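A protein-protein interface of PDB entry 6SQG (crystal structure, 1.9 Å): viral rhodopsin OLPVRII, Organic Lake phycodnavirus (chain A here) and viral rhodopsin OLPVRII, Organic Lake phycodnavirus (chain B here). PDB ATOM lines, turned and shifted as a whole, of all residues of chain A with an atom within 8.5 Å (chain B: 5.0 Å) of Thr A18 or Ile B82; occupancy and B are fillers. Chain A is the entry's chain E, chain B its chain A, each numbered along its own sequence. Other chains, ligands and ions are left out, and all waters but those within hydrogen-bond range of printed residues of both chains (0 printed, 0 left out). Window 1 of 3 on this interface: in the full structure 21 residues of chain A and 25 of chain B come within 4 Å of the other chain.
The backbone carbonyl oxygen (O) of Thr A18 is in hydrogen-bond range of the side-chain sulfur (SG) of Cys B44, at 3.7 Å.
Thr A18 touches just these residues of chain B: Cys B44 (3.7 Å), Val B48 (2.9 Å), Ile B78 (3.8 Å) and Ile B82 (3.8 Å).
Of chain A, only Thr A18 (3.8 Å) comes within 4 Å of Ile B82.
No residue of chain A comes within 4 Å of Pro B81.
Of the printed residues of chain A, Leu B41 touches Ile A22 (3.5 Å) and Trp A203 (3.8 Å).
Of the printed residues of chain A, Val B48 touches Ala A14 (3.9 Å) and Thr A18 (2.9 Å).
Printed residues of chain B within 4 Å of Ile A22: Leu B41 and Cys B44.
Printed residues of chain B within 4 Å of Trp A203: Leu B41 (3.8 Å).
Printed residues of chain A within 4 Å of Ile B78: Leu A11, Ala A14, Phe A15 and Thr A18.
The nearest printed residue of chain B that does not touch Thr A18 is Ile B45 (6.1 Å).
The nearest residue of chain A that does not touch Ile B82 is Phe A15 (5.3 Å).
The nearest printed residue of chain A that does not touch Leu B41 is Ile A25 (6.2 Å).
Among the printed residues, merely in contact across the chains: Leu A11 with Ile B78 (3.7 Å), Ala A14 with Val B48 (3.9 Å), Ala A14 with Ile B78 (3.3 Å), Phe A15 with Ile B78 (3.8 Å), Thr A18 with Val B48 (2.9 Å), Thr A18 with Ile B78 (3.8 Å), Thr A18 with Ile B82 (3.8 Å), Thr A21 with Cys B44 (3.9 Å), Ile A22 with Leu B41 (3.5 Å), Ile A22 with Cys B44 (3.8 Å) and Trp A203 with Leu B41 (3.8 Å).
Hydrophobic or aromatic side chains of chain B within 4 Å of the printed part of chain A: Leu B41, Val B48, Ile B78 and Ile B82.
Hydrophobic or aromatic side chains of chain A that line the printed part of chain B: Leu A11, Ala A14, Phe A15, Ile A22 and Trp A203.
Among the printed residues, no Asp or Glu carboxylate lies within 4 Å of a Lys or Arg side-chain nitrogen of the other chain.
The backbone carbonyl oxygen (O) of Ala A14 sits at hydrogen-bond distance from the side-chain hydroxyl (OG1) of Thr A18 (3.2 Å).
O of Phe A15 is in hydrogen-bond range of OG1 of Thr A19, 2.9 Å away.
The side-chain sulfur (SG) of Cys A196 sits close to the backbone carbonyl oxygen (O) of Phe A15 (3.7 Å).
The backbone carbonyl oxygen of Met A17 lies within hydrogen-bond range of the side-chain hydroxyl of Thr A21, 2.8 Å away.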
ATOM      1  N   LEU A  11      -1.682   8.346 -14.291  1.00  0.00           N
ATOM      2  CA  LEU A  11      -1.516   7.216 -15.185  1.00  0.00           C
ATOM      3  C   LEU A  11      -0.286   7.417 -16.065  1.00  0.00           C
ATOM      4  O   LEU A  11       0.538   6.525 -16.218  1.00  0.00           O
ATOM      5  CB  LEU A  11      -2.771   7.028 -16.052  1.00  0.00           C
ATOM      6  CG  LEU A  11      -2.710   5.908 -17.098  1.00  0.00           C
ATOM      7  CD1 LEU A  11      -2.632   4.536 -16.439  1.00  0.00           C
ATOM      8  CD2 LEU A  11      -3.918   5.984 -18.020  1.00  0.00           C
ATOM      9  N   THR A  12      -0.155   8.612 -16.628  1.00  0.00           N
ATOM     10  CA  THR A  12       0.972   8.905 -17.494  1.00  0.00           C
ATOM     11  C   THR A  12       2.272   8.982 -16.702  1.00  0.00           C
ATOM     12  O   THR A  12       3.296   8.447 -17.134  1.00  0.00           O
ATOM     13  CB  THR A  12       0.709  10.180 -18.299  1.00  0.00           C
ATOM     14  OG1 THR A  12      -0.405   9.941 -19.174  1.00  0.00           O
ATOM     15  CG2 THR A  12       1.943  10.576 -19.122  1.00  0.00           C
ATOM     16  N   TYR A  13       2.228   9.633 -15.544  1.00  0.00           N
ATOM     17  CA  TYR A  13       3.398   9.717 -14.657  1.00  0.00           C
ATOM     18  C   TYR A  13       3.931   8.329 -14.302  1.00  0.00           C
ATOM     19  O   TYR A  13       5.131   8.054 -14.424  1.00  0.00           O
ATOM     20  CB  TYR A  13       3.035  10.507 -13.399  1.00  0.00           C
ATOM     21  CG  TYR A  13       4.186  10.780 -12.466  1.00  0.00           C
ATOM     22  CD1 TYR A  13       5.437  11.152 -12.954  1.00  0.00           C
ATOM     23  CD2 TYR A  13       4.025  10.687 -11.095  1.00  0.00           C
ATOM     24  CE1 TYR A  13       6.495  11.400 -12.102  1.00  0.00           C
ATOM     25  CE2 TYR A  13       5.075  10.944 -10.232  1.00  0.00           C
ATOM     26  CZ  TYR A  13       6.309  11.296 -10.743  1.00  0.00           C
ATOM     27  OH  TYR A  13       7.360  11.542  -9.888  1.00  0.00           O
ATOM     28  N   ALA A  14       3.045   7.442 -13.873  1.00  0.00           N
ATOM     29  CA  ALA A  14       3.460   6.099 -13.489  1.00  0.00           C
ATOM     30  C   ALA A  14       3.925   5.276 -14.701  1.00  0.00           C
ATOM     31  O   ALA A  14       4.891   4.541 -14.608  1.00  0.00           O
ATOM     32  CB  ALA A  14       2.340   5.391 -12.739  1.00  0.00           C
ATOM     33  N   PHE A  15       3.266   5.412 -15.848  1.00  0.00           N
ATOM     34  CA  PHE A  15       3.734   4.714 -17.035  1.00  0.00           C
ATOM     35  C   PHE A  15       5.079   5.263 -17.539  1.00  0.00           C
ATOM     36  O   PHE A  15       5.857   4.518 -18.130  1.00  0.00           O
ATOM     37  CB  PHE A  15       2.691   4.714 -18.163  1.00  0.00           C
ATOM     38  CG  PHE A  15       2.112   3.357 -18.449  1.00  0.00           C
ATOM     39  CD1 PHE A  15       2.918   2.328 -18.924  1.00  0.00           C
ATOM     40  CD2 PHE A  15       0.763   3.103 -18.242  1.00  0.00           C
ATOM     41  CE1 PHE A  15       2.392   1.073 -19.182  1.00  0.00           C
ATOM     42  CE2 PHE A  15       0.228   1.850 -18.505  1.00  0.00           C
ATOM     43  CZ  PHE A  15       1.044   0.832 -18.974  1.00  0.00           C
ATOM     44  N   LEU A  16       5.360   6.545 -17.305  1.00  0.00           N
ATOM     45  CA  LEU A  16       6.700   7.082 -17.621  1.00  0.00           C
ATOM     46  C   LEU A  16       7.794   6.445 -16.741  1.00  0.00           C
ATOM     47  O   LEU A  16       8.906   6.171 -17.200  1.00  0.00           O
ATOM     48  CB  LEU A  16       6.729   8.606 -17.496  1.00  0.00           C
ATOM     49  CG  LEU A  16       6.038   9.361 -18.641  1.00  0.00           C
ATOM     50  CD1 LEU A  16       5.716  10.780 -18.203  1.00  0.00           C
ATOM     51  CD2 LEU A  16       6.868   9.353 -19.910  1.00  0.00           C
ATOM     52  N   MET A  17       7.484   6.204 -15.475  1.00  0.00           N
ATOM     53  CA  MET A  17       8.414   5.488 -14.593  1.00  0.00           C
ATOM     54  C   MET A  17       8.644   4.061 -15.080  1.00  0.00           C
ATOM     55  O   MET A  17       9.758   3.540 -14.993  1.00  0.00           O
ATOM     56  CB  MET A  17       7.881   5.437 -13.166  1.00  0.00           C
ATOM     57  CG  MET A  17       7.798   6.777 -12.461  1.00  0.00           C
ATOM     58  SD  MET A  17       7.216   6.541 -10.765  1.00  0.00           S
ATOM     59  CE  MET A  17       6.575   8.181 -10.429  1.00  0.00           C
ATOM     60  N   THR A  18       7.588   3.426 -15.584  1.00  0.00           N
ATOM     61  CA  THR A  18       7.685   2.065 -16.122  1.00  0.00           C
ATOM     62  C   THR A  18       8.561   2.065 -17.366  1.00  0.00           C
ATOM     63  O   THR A  18       9.490   1.280 -17.494  1.00  0.00           O
ATOM     64  CB  THR A  18       6.279   1.506 -16.488  1.00  0.00           C
ATOM     65  OG1 THR A  18       5.443   1.489 -15.323  1.00  0.00           O
ATOM     66  CG2 THR A  18       6.362   0.102 -17.067  1.00  0.00           C
ATOM     67  N   THR A  19       8.255   2.958 -18.298  1.00  0.00           N
ATOM     68  CA  THR A  19       8.984   3.004 -19.547  1.00  0.00           C
ATOM     69  C   THR A  19      10.457   3.348 -19.311  1.00  0.00           C
ATOM     70  O   THR A  19      11.347   2.749 -19.906  1.00  0.00           O
ATOM     71  CB  THR A  19       8.348   4.008 -20.523  1.00  0.00           C
ATOM     72  OG1 THR A  19       6.965   3.667 -20.724  1.00  0.00           O
ATOM     73  CG2 THR A  19       9.072   3.969 -21.850  1.00  0.00           C
ATOM     74  N   GLY A  20      10.711   4.302 -18.430  1.00  0.00           N
ATOM     75  CA  GLY A  20      12.079   4.679 -18.102  1.00  0.00           C
ATOM     76  C   GLY A  20      12.877   3.534 -17.504  1.00  0.00           C
ATOM     77  O   GLY A  20      14.048   3.354 -17.816  1.00  0.00           O
ATOM     78  N   THR A  21      12.242   2.739 -16.655  1.00  0.00           N
ATOM     79  CA  THR A  21      12.927   1.617 -16.014  1.00  0.00           C
ATOM     80  C   THR A  21      13.282   0.514 -17.000  1.00  0.00           C
ATOM     81  O   THR A  21      14.401  -0.003 -17.007  1.00  0.00           O
ATOM     82  CB  THR A  21      12.049   1.002 -14.910  1.00  0.00           C
ATOM     83  OG1 THR A  21      11.783   2.003 -13.918  1.00  0.00           O
ATOM     84  CG2 THR A  21      12.748  -0.189 -14.266  1.00  0.00           C
ATOM     85  N   ILE A  22      12.329   0.183 -17.855  1.00  0.00           N
ATOM     86  CA  ILE A  22      12.474  -0.931 -18.765  1.00  0.00           C
ATOM     87  C   ILE A  22      13.559  -0.628 -19.810  1.00  0.00           C
ATOM     88  O   ILE A  22      14.372  -1.491 -20.132  1.00  0.00           O
ATOM     89  CB  ILE A  22      11.100  -1.317 -19.379  1.00  0.00           C
ATOM     90  CG1 ILE A  22      11.053  -2.810 -19.706  1.00  0.00           C
ATOM     91  CG2 ILE A  22      10.758  -0.471 -20.599  1.00  0.00           C
ATOM     92  CD1 ILE A  22       9.663  -3.296 -20.044  1.00  0.00           C
ATOM     93  N   THR A  23      13.599   0.604 -20.307  1.00  0.00           N
ATOM     94  CA  THR A  23      14.615   0.982 -21.297  1.00  0.00           C
ATOM     95  C   THR A  23      16.007   1.185 -20.645  1.00  0.00           C
ATOM     96  O   THR A  23      17.047   0.874 -21.245  1.00  0.00           O
ATOM     97  CB  THR A  23      14.197   2.245 -22.103  1.00  0.00           C
ATOM     98  OG1 THR A  23      13.988   3.360 -21.221  1.00  0.00           O
ATOM     99  CG2 THR A  23      12.906   1.990 -22.876  1.00  0.00           C
ATOM    100  N   PHE A  24      16.020   1.712 -19.426  1.00  0.00           N
ATOM    101  CA  PHE A  24      17.246   1.830 -18.648  1.00  0.00           C
ATOM    102  C   PHE A  24      17.944   0.487 -18.494  1.00  0.00           C
ATOM    103  O   PHE A  24      19.130   0.341 -18.812  1.00  0.00           O
ATOM    104  CB  PHE A  24      16.938   2.420 -17.281  1.00  0.00           C
ATOM    105  CG  PHE A  24      18.139   2.631 -16.415  1.00  0.00           C
ATOM    106  CD1 PHE A  24      19.146   3.504 -16.795  1.00  0.00           C
ATOM    107  CD2 PHE A  24      18.249   1.986 -15.197  1.00  0.00           C
ATOM    108  CE1 PHE A  24      20.248   3.715 -15.987  1.00  0.00           C
ATOM    109  CE2 PHE A  24      19.340   2.199 -14.381  1.00  0.00           C
ATOM    110  CZ  PHE A  24      20.342   3.067 -14.774  1.00  0.00           C
ATOM    111  N   ILE A  25      17.212  -0.502 -18.005  1.00  0.00           N
ATOM    112  CA  ILE A  25      17.814  -1.801 -17.723  1.00  0.00           C
ATOM    113  C   ILE A  25      18.325  -2.460 -19.008  1.00  0.00           C
ATOM    114  O   ILE A  25      19.431  -3.010 -19.049  1.00  0.00           O
ATOM    115  CB  ILE A  25      16.834  -2.713 -16.963  1.00  0.00           C
ATOM    116  CG1 ILE A  25      16.671  -2.207 -15.530  1.00  0.00           C
ATOM    117  CG2 ILE A  25      17.319  -4.155 -16.986  1.00  0.00           C
ATOM    118  CD1 ILE A  25      15.560  -2.887 -14.762  1.00  0.00           C
ATOM    119  N   THR A  43      15.250   6.413 -22.534  1.00  0.00           N
ATOM    120  CA  THR A  43      15.278   6.610 -21.079  1.00  0.00           C
ATOM    121  C   THR A  43      15.246   8.100 -20.738  1.00  0.00           C
ATOM    122  O   THR A  43      14.512   8.521 -19.844  1.00  0.00           O
ATOM    123  CB  THR A  43      16.523   5.937 -20.447  1.00  0.00           C
ATOM    124  OG1 THR A  43      16.562   4.555 -20.804  1.00  0.00           O
ATOM    125  CG2 THR A  43      16.524   6.044 -18.953  1.00  0.00           C
ATOM    126  N   SER A  46      11.742   9.601 -20.956  1.00  0.00           N
ATOM    127  CA  SER A  46      10.954   9.269 -19.768  1.00  0.00           C
ATOM    128  C   SER A  46      11.379  10.053 -18.526  1.00  0.00           C
ATOM    129  O   SER A  46      10.541  10.483 -17.738  1.00  0.00           O
ATOM    130  CB  SER A  46      11.046   7.771 -19.487  1.00  0.00           C
ATOM    131  OG  SER A  46      10.363   7.047 -20.490  1.00  0.00           O
ATOM    132  N   ALA A  50       8.771  12.622 -16.967  1.00  0.00           N
ATOM    133  CA  ALA A  50       8.403  12.323 -15.581  1.00  0.00           C
ATOM    134  C   ALA A  50       8.617  13.527 -14.665  1.00  0.00           C
ATOM    135  O   ALA A  50       7.788  13.809 -13.815  1.00  0.00           O
ATOM    136  CB  ALA A  50       9.186  11.136 -15.062  1.00  0.00           C
ATOM    137  N   LEU A 192       0.992   9.405 -23.031  1.00  0.00           N
ATOM    138  CA  LEU A 192       1.028   7.986 -22.675  1.00  0.00           C
ATOM    139  C   LEU A 192       1.334   7.149 -23.911  1.00  0.00           C
ATOM    140  O   LEU A 192       2.149   6.220 -23.866  1.00  0.00           O
ATOM    141  CB  LEU A 192      -0.302   7.566 -22.048  1.00  0.00           C
ATOM    142  CG  LEU A 192      -0.512   6.091 -21.725  1.00  0.00           C
ATOM    143  CD1 LEU A 192       0.299   5.707 -20.503  1.00  0.00           C
ATOM    144  CD2 LEU A 192      -1.985   5.774 -21.497  1.00  0.00           C
ATOM    145  N   CYS A 196       5.324   6.739 -23.727  1.00  0.00           N
ATOM    146  CA  CYS A 196       5.389   5.439 -23.039  1.00  0.00           C
ATOM    147  C   CYS A 196       5.165   4.225 -23.931  1.00  0.00           C
ATOM    148  O   CYS A 196       5.972   3.310 -23.937  1.00  0.00           O
ATOM    149  CB  CYS A 196       4.392   5.380 -21.890  1.00  0.00           C
ATOM    150  SG  CYS A 196       4.499   6.768 -20.755  1.00  0.00           S
ATOM    151  N   PHE A 197       4.061   4.186 -24.669  1.00  0.00           N
ATOM    152  CA  PHE A 197       3.777   3.000 -25.473  1.00  0.00           C
ATOM    153  C   PHE A 197       4.797   2.859 -26.596  1.00  0.00           C
ATOM    154  O   PHE A 197       5.216   1.752 -26.923  1.00  0.00           O
ATOM    155  CB  PHE A 197       2.354   3.000 -26.021  1.00  0.00           C
ATOM    156  CG  PHE A 197       1.297   2.843 -24.965  1.00  0.00           C
ATOM    157  CD1 PHE A 197       1.640   2.612 -23.641  1.00  0.00           C
ATOM    158  CD2 PHE A 197      -0.042   2.890 -25.308  1.00  0.00           C
ATOM    159  CE1 PHE A 197       0.661   2.464 -22.673  1.00  0.00           C
ATOM    160  CE2 PHE A 197      -1.023   2.737 -24.347  1.00  0.00           C
ATOM    161  CZ  PHE A 197      -0.672   2.517 -23.031  1.00  0.00           C
ATOM    162  N   GLY A 199       7.990   3.937 -26.355  1.00  0.00           N
ATOM    163  CA  GLY A 199       9.149   3.400 -25.633  1.00  0.00           C
ATOM    164  C   GLY A 199       9.045   1.900 -25.368  1.00  0.00           C
ATOM    165  O   GLY A 199       9.995   1.134 -25.573  1.00  0.00           O
ATOM    166  N   ILE A 200       7.888   1.476 -24.891  1.00  0.00           N
ATOM    167  CA  ILE A 200       7.677   0.068 -24.573  1.00  0.00           C
ATOM    168  C   ILE A 200       7.744  -0.760 -25.857  1.00  0.00           C
ATOM    169  O   ILE A 200       8.294  -1.860 -25.867  1.00  0.00           O
ATOM    170  CB  ILE A 200       6.356  -0.137 -23.818  1.00  0.00           C
ATOM    171  CG1 ILE A 200       6.456   0.480 -22.421  1.00  0.00           C
ATOM    172  CG2 ILE A 200       6.018  -1.619 -23.704  1.00  0.00           C
ATOM    173  CD1 ILE A 200       5.139   0.572 -21.682  1.00  0.00           C
ATOM    174  N   TRP A 203      11.456  -1.288 -26.714  1.00  0.00           N
ATOM    175  CA  TRP A 203      12.011  -2.333 -25.865  1.00  0.00           C
ATOM    176  C   TRP A 203      11.559  -3.725 -26.331  1.00  0.00           C
ATOM    177  O   TRP A 203      12.377  -4.620 -26.572  1.00  0.00           O
ATOM    178  CB  TRP A 203      11.583  -2.114 -24.419  1.00  0.00           C
ATOM    179  CG  TRP A 203      11.924  -3.282 -23.574  1.00  0.00           C
ATOM    180  CD1 TRP A 203      13.148  -3.586 -23.062  1.00  0.00           C
ATOM    181  CD2 TRP A 203      11.039  -4.319 -23.150  1.00  0.00           C
ATOM    182  NE1 TRP A 203      13.083  -4.754 -22.349  1.00  0.00           N
ATOM    183  CE2 TRP A 203      11.797  -5.224 -22.385  1.00  0.00           C
ATOM    184  CE3 TRP A 203       9.685  -4.578 -23.350  1.00  0.00           C
ATOM    185  CZ2 TRP A 203      11.244  -6.365 -21.820  1.00  0.00           C
ATOM    186  CZ3 TRP A 203       9.138  -5.726 -22.794  1.00  0.00           C
ATOM    187  CH2 TRP A 203       9.914  -6.594 -22.033  1.00  0.00           C
ATOM    188  N   LEU B  41      10.771  -6.581 -16.267  1.00  0.00           N
ATOM    189  CA  LEU B  41       9.341  -6.365 -16.089  1.00  0.00           C
ATOM    190  C   LEU B  41       8.943  -6.409 -14.606  1.00  0.00           C
ATOM    191  O   LEU B  41       8.194  -5.547 -14.131  1.00  0.00           O
ATOM    192  CB  LEU B  41       8.530  -7.381 -16.900  1.00  0.00           C
ATOM    193  CG  LEU B  41       8.613  -7.253 -18.423  1.00  0.00           C
ATOM    194  CD1 LEU B  41       8.141  -8.529 -19.117  1.00  0.00           C
ATOM    195  CD2 LEU B  41       7.813  -6.064 -18.915  1.00  0.00           C
ATOM    196  N   CYS B  44       9.789  -3.239 -12.929  1.00  0.00           N
ATOM    197  CA  CYS B  44       8.809  -2.207 -13.259  1.00  0.00           C
ATOM    198  C   CYS B  44       7.603  -2.287 -12.340  1.00  0.00           C
ATOM    199  O   CYS B  44       7.137  -1.278 -11.824  1.00  0.00           O
ATOM    200  CB  CYS B  44       8.354  -2.319 -14.719  1.00  0.00           C
ATOM    201  SG  CYS B  44       9.702  -2.000 -15.879  1.00  0.00           S
ATOM    202  N   ILE B  45       7.103  -3.498 -12.136  1.00  0.00           N
ATOM    203  CA  ILE B  45       5.967  -3.707 -11.259  1.00  0.00           C
ATOM    204  C   ILE B  45       6.207  -3.119  -9.870  1.00  0.00           C
ATOM    205  O   ILE B  45       5.359  -2.381  -9.358  1.00  0.00           O
ATOM    206  CB  ILE B  45       5.605  -5.203 -11.163  1.00  0.00           C
ATOM    207  CG1 ILE B  45       5.025  -5.686 -12.489  1.00  0.00           C
ATOM    208  CG2 ILE B  45       4.570  -5.446 -10.071  1.00  0.00           C
ATOM    209  CD1 ILE B  45       5.100  -7.187 -12.668  1.00  0.00           C
ATOM    210  N   VAL B  48       6.361   0.833  -9.918  1.00  0.00           N
ATOM    211  CA  VAL B  48       5.052   1.459 -10.012  1.00  0.00           C
ATOM    212  C   VAL B  48       4.246   1.309  -8.727  1.00  0.00           C
ATOM    213  O   VAL B  48       3.703   2.298  -8.210  1.00  0.00           O
ATOM    214  CB  VAL B  48       4.237   0.866 -11.180  1.00  0.00           C
ATOM    215  CG1 VAL B  48       2.774   1.267 -11.082  1.00  0.00           C
ATOM    216  CG2 VAL B  48       4.829   1.321 -12.495  1.00  0.00           C
ATOM    217  N   ILE B  78      -1.867  -0.349 -14.563  1.00  0.00           N
ATOM    218  CA  ILE B  78      -0.489  -0.380 -15.040  1.00  0.00           C
ATOM    219  C   ILE B  78       0.186  -1.699 -14.688  1.00  0.00           C
ATOM    220  O   ILE B  78       0.874  -2.303 -15.513  1.00  0.00           O
ATOM    221  CB  ILE B  78       0.300   0.801 -14.445  1.00  0.00           C
ATOM    222  CG1 ILE B  78      -0.412   2.113 -14.798  1.00  0.00           C
ATOM    223  CG2 ILE B  78       1.740   0.793 -14.944  1.00  0.00           C
ATOM    224  CD1 ILE B  78       0.164   3.337 -14.113  1.00  0.00           C
ATOM    225  N   THR B  79      -0.029  -2.169 -13.465  1.00  0.00           N
ATOM    226  CA  THR B  79       0.705  -3.323 -12.997  1.00  0.00           C
ATOM    227  C   THR B  79       0.134  -4.642 -13.497  1.00  0.00           C
ATOM    228  O   THR B  79       0.898  -5.531 -13.848  1.00  0.00           O
ATOM    229  CB  THR B  79       0.840  -3.335 -11.470  1.00  0.00           C
ATOM    230  OG1 THR B  79      -0.460  -3.317 -10.866  1.00  0.00           O
ATOM    231  CG2 THR B  79       1.642  -2.125 -11.015  1.00  0.00           C
ATOM    232  N   THR B  80      -1.194  -4.769 -13.573  1.00  0.00           N
ATOM    233  CA  THR B  80      -1.762  -6.032 -14.022  1.00  0.00           C
ATOM    234  C   THR B  80      -1.297  -6.473 -15.415  1.00  0.00           C
ATOM    235  O   THR B  80      -0.982  -7.638 -15.599  1.00  0.00           O
ATOM    236  CB  THR B  80      -3.301  -6.085 -13.894  1.00  0.00           C
ATOM    237  OG1 THR B  80      -3.910  -5.042 -14.654  1.00  0.00           O
ATOM    238  CG2 THR B  80      -3.708  -5.959 -12.427  1.00  0.00           C
ATOM    239  N   PRO B  81      -1.253  -5.565 -16.400  1.00  0.00           N
ATOM    240  CA  PRO B  81      -0.766  -6.047 -17.703  1.00  0.00           C
ATOM    241  C   PRO B  81       0.698  -6.499 -17.703  1.00  0.00           C
ATOM    242  O   PRO B  81       1.064  -7.435 -18.437  1.00  0.00           O
ATOM    243  CB  PRO B  81      -0.939  -4.829 -18.630  1.00  0.00           C
ATOM    244  CG  PRO B  81      -1.071  -3.650 -17.717  1.00  0.00           C
ATOM    245  CD  PRO B  81      -1.730  -4.176 -16.470  1.00  0.00           C
ATOM    246  N   ILE B  82       1.535  -5.836 -16.911  1.00  0.00           N
ATOM    247  CA  ILE B  82       2.941  -6.216 -16.835  1.00  0.00           C
ATOM    248  C   ILE B  82       3.071  -7.581 -16.150  1.00  0.00           C
ATOM    249  O   ILE B  82       3.832  -8.442 -16.602  1.00  0.00           O
ATOM    250  CB  ILE B  82       3.777  -5.170 -16.080  1.00  0.00           C
ATOM    251  CG1 ILE B  82       3.607  -3.777 -16.701  1.00  0.00           C
ATOM    252  CG2 ILE B  82       5.236  -5.574 -16.096  1.00  0.00           C
ATOM    253  CD1 ILE B  82       4.063  -2.661 -15.786  1.00  0.00           C
ATOM    254  N   MET B  83       2.325  -7.765 -15.064  1.00  0.00           N
ATOM    255  CA  MET B  83       2.285  -9.039 -14.340  1.00  0.00           C
ATOM    256  C   MET B  83       1.843 -10.209 -15.221  1.00  0.00           C
ATOM    257  O   MET B  83       2.401 -11.306 -15.136  1.00  0.00           O
ATOM    258  CB  MET B  83       1.346  -8.931 -13.136  1.00  0.00           C
ATOM    259  CG  MET B  83       1.863  -8.007 -12.041  1.00  0.00           C
ATOM    260  SD  MET B  83       0.602  -7.580 -10.830  1.00  0.00           S
ATOM    261  CE  MET B  83       0.600  -9.077  -9.852  1.00  0.00           C
ATOM    262  N   LEU B  84       0.848  -9.968 -16.070  1.00  0.00           N
ATOM    263  CA  LEU B  84       0.340 -11.002 -16.973  1.00  0.00           C
ATOM    264  C   LEU B  84       1.340 -11.299 -18.085  1.00  0.00           C
ATOM    265  O   LEU B  84       1.482 -12.439 -18.509  1.00  0.00           O
ATOM    266  CB  LEU B  84      -0.996 -10.554 -17.570  1.00  0.00           C
ATOM    267  CG  LEU B  84      -2.140 -10.474 -16.558  1.00  0.00           C
ATOM    268  CD1 LEU B  84      -3.342  -9.774 -17.164  1.00  0.00           C
ATOM    269  CD2 LEU B  84      -2.510 -11.853 -16.049  1.00  0.00           C
ATOM    270  N   LEU B  85       2.030 -10.267 -18.555  1.00  0.00           N
ATOM    271  CA  LEU B  85       3.071 -10.439 -19.564  1.00  0.00           C
ATOM    272  C   LEU B  85       4.158 -11.319 -18.987  1.00  0.00           C
ATOM    273  O   LEU B  85       4.575 -12.310 -19.600  1.00  0.00           O
ATOM    274  CB  LEU B  85       3.641  -9.093 -20.015  1.00  0.00           C
ATOM    275  CG  LEU B  85       4.749  -9.171 -21.073  1.00  0.00           C
ATOM    276  CD1 LEU B  85       4.289  -9.967 -22.285  1.00  0.00           C
ATOM    277  CD2 LEU B  85       5.188  -7.782 -21.494  1.00  0.00           C
ATOM    278  N   VAL B  86       4.599 -10.983 -17.785  1.00  0.00           N
ATOM    279  CA  VAL B  86       5.566 -11.829 -17.070  1.00  0.00           C
ATOM    280  C   VAL B  86       5.088 -13.279 -16.982  1.00  0.00           C
ATOM    281  O   VAL B  86       5.833 -14.202 -17.286  1.00  0.00           O
ATOM    282  CB  VAL B  86       5.847 -11.281 -15.661  1.00  0.00           C
ATOM    283  CG1 VAL B  86       6.605 -12.302 -14.821  1.00  0.00           C
ATOM    284  CG2 VAL B  86       6.642  -9.986 -15.757  1.00  0.00           C
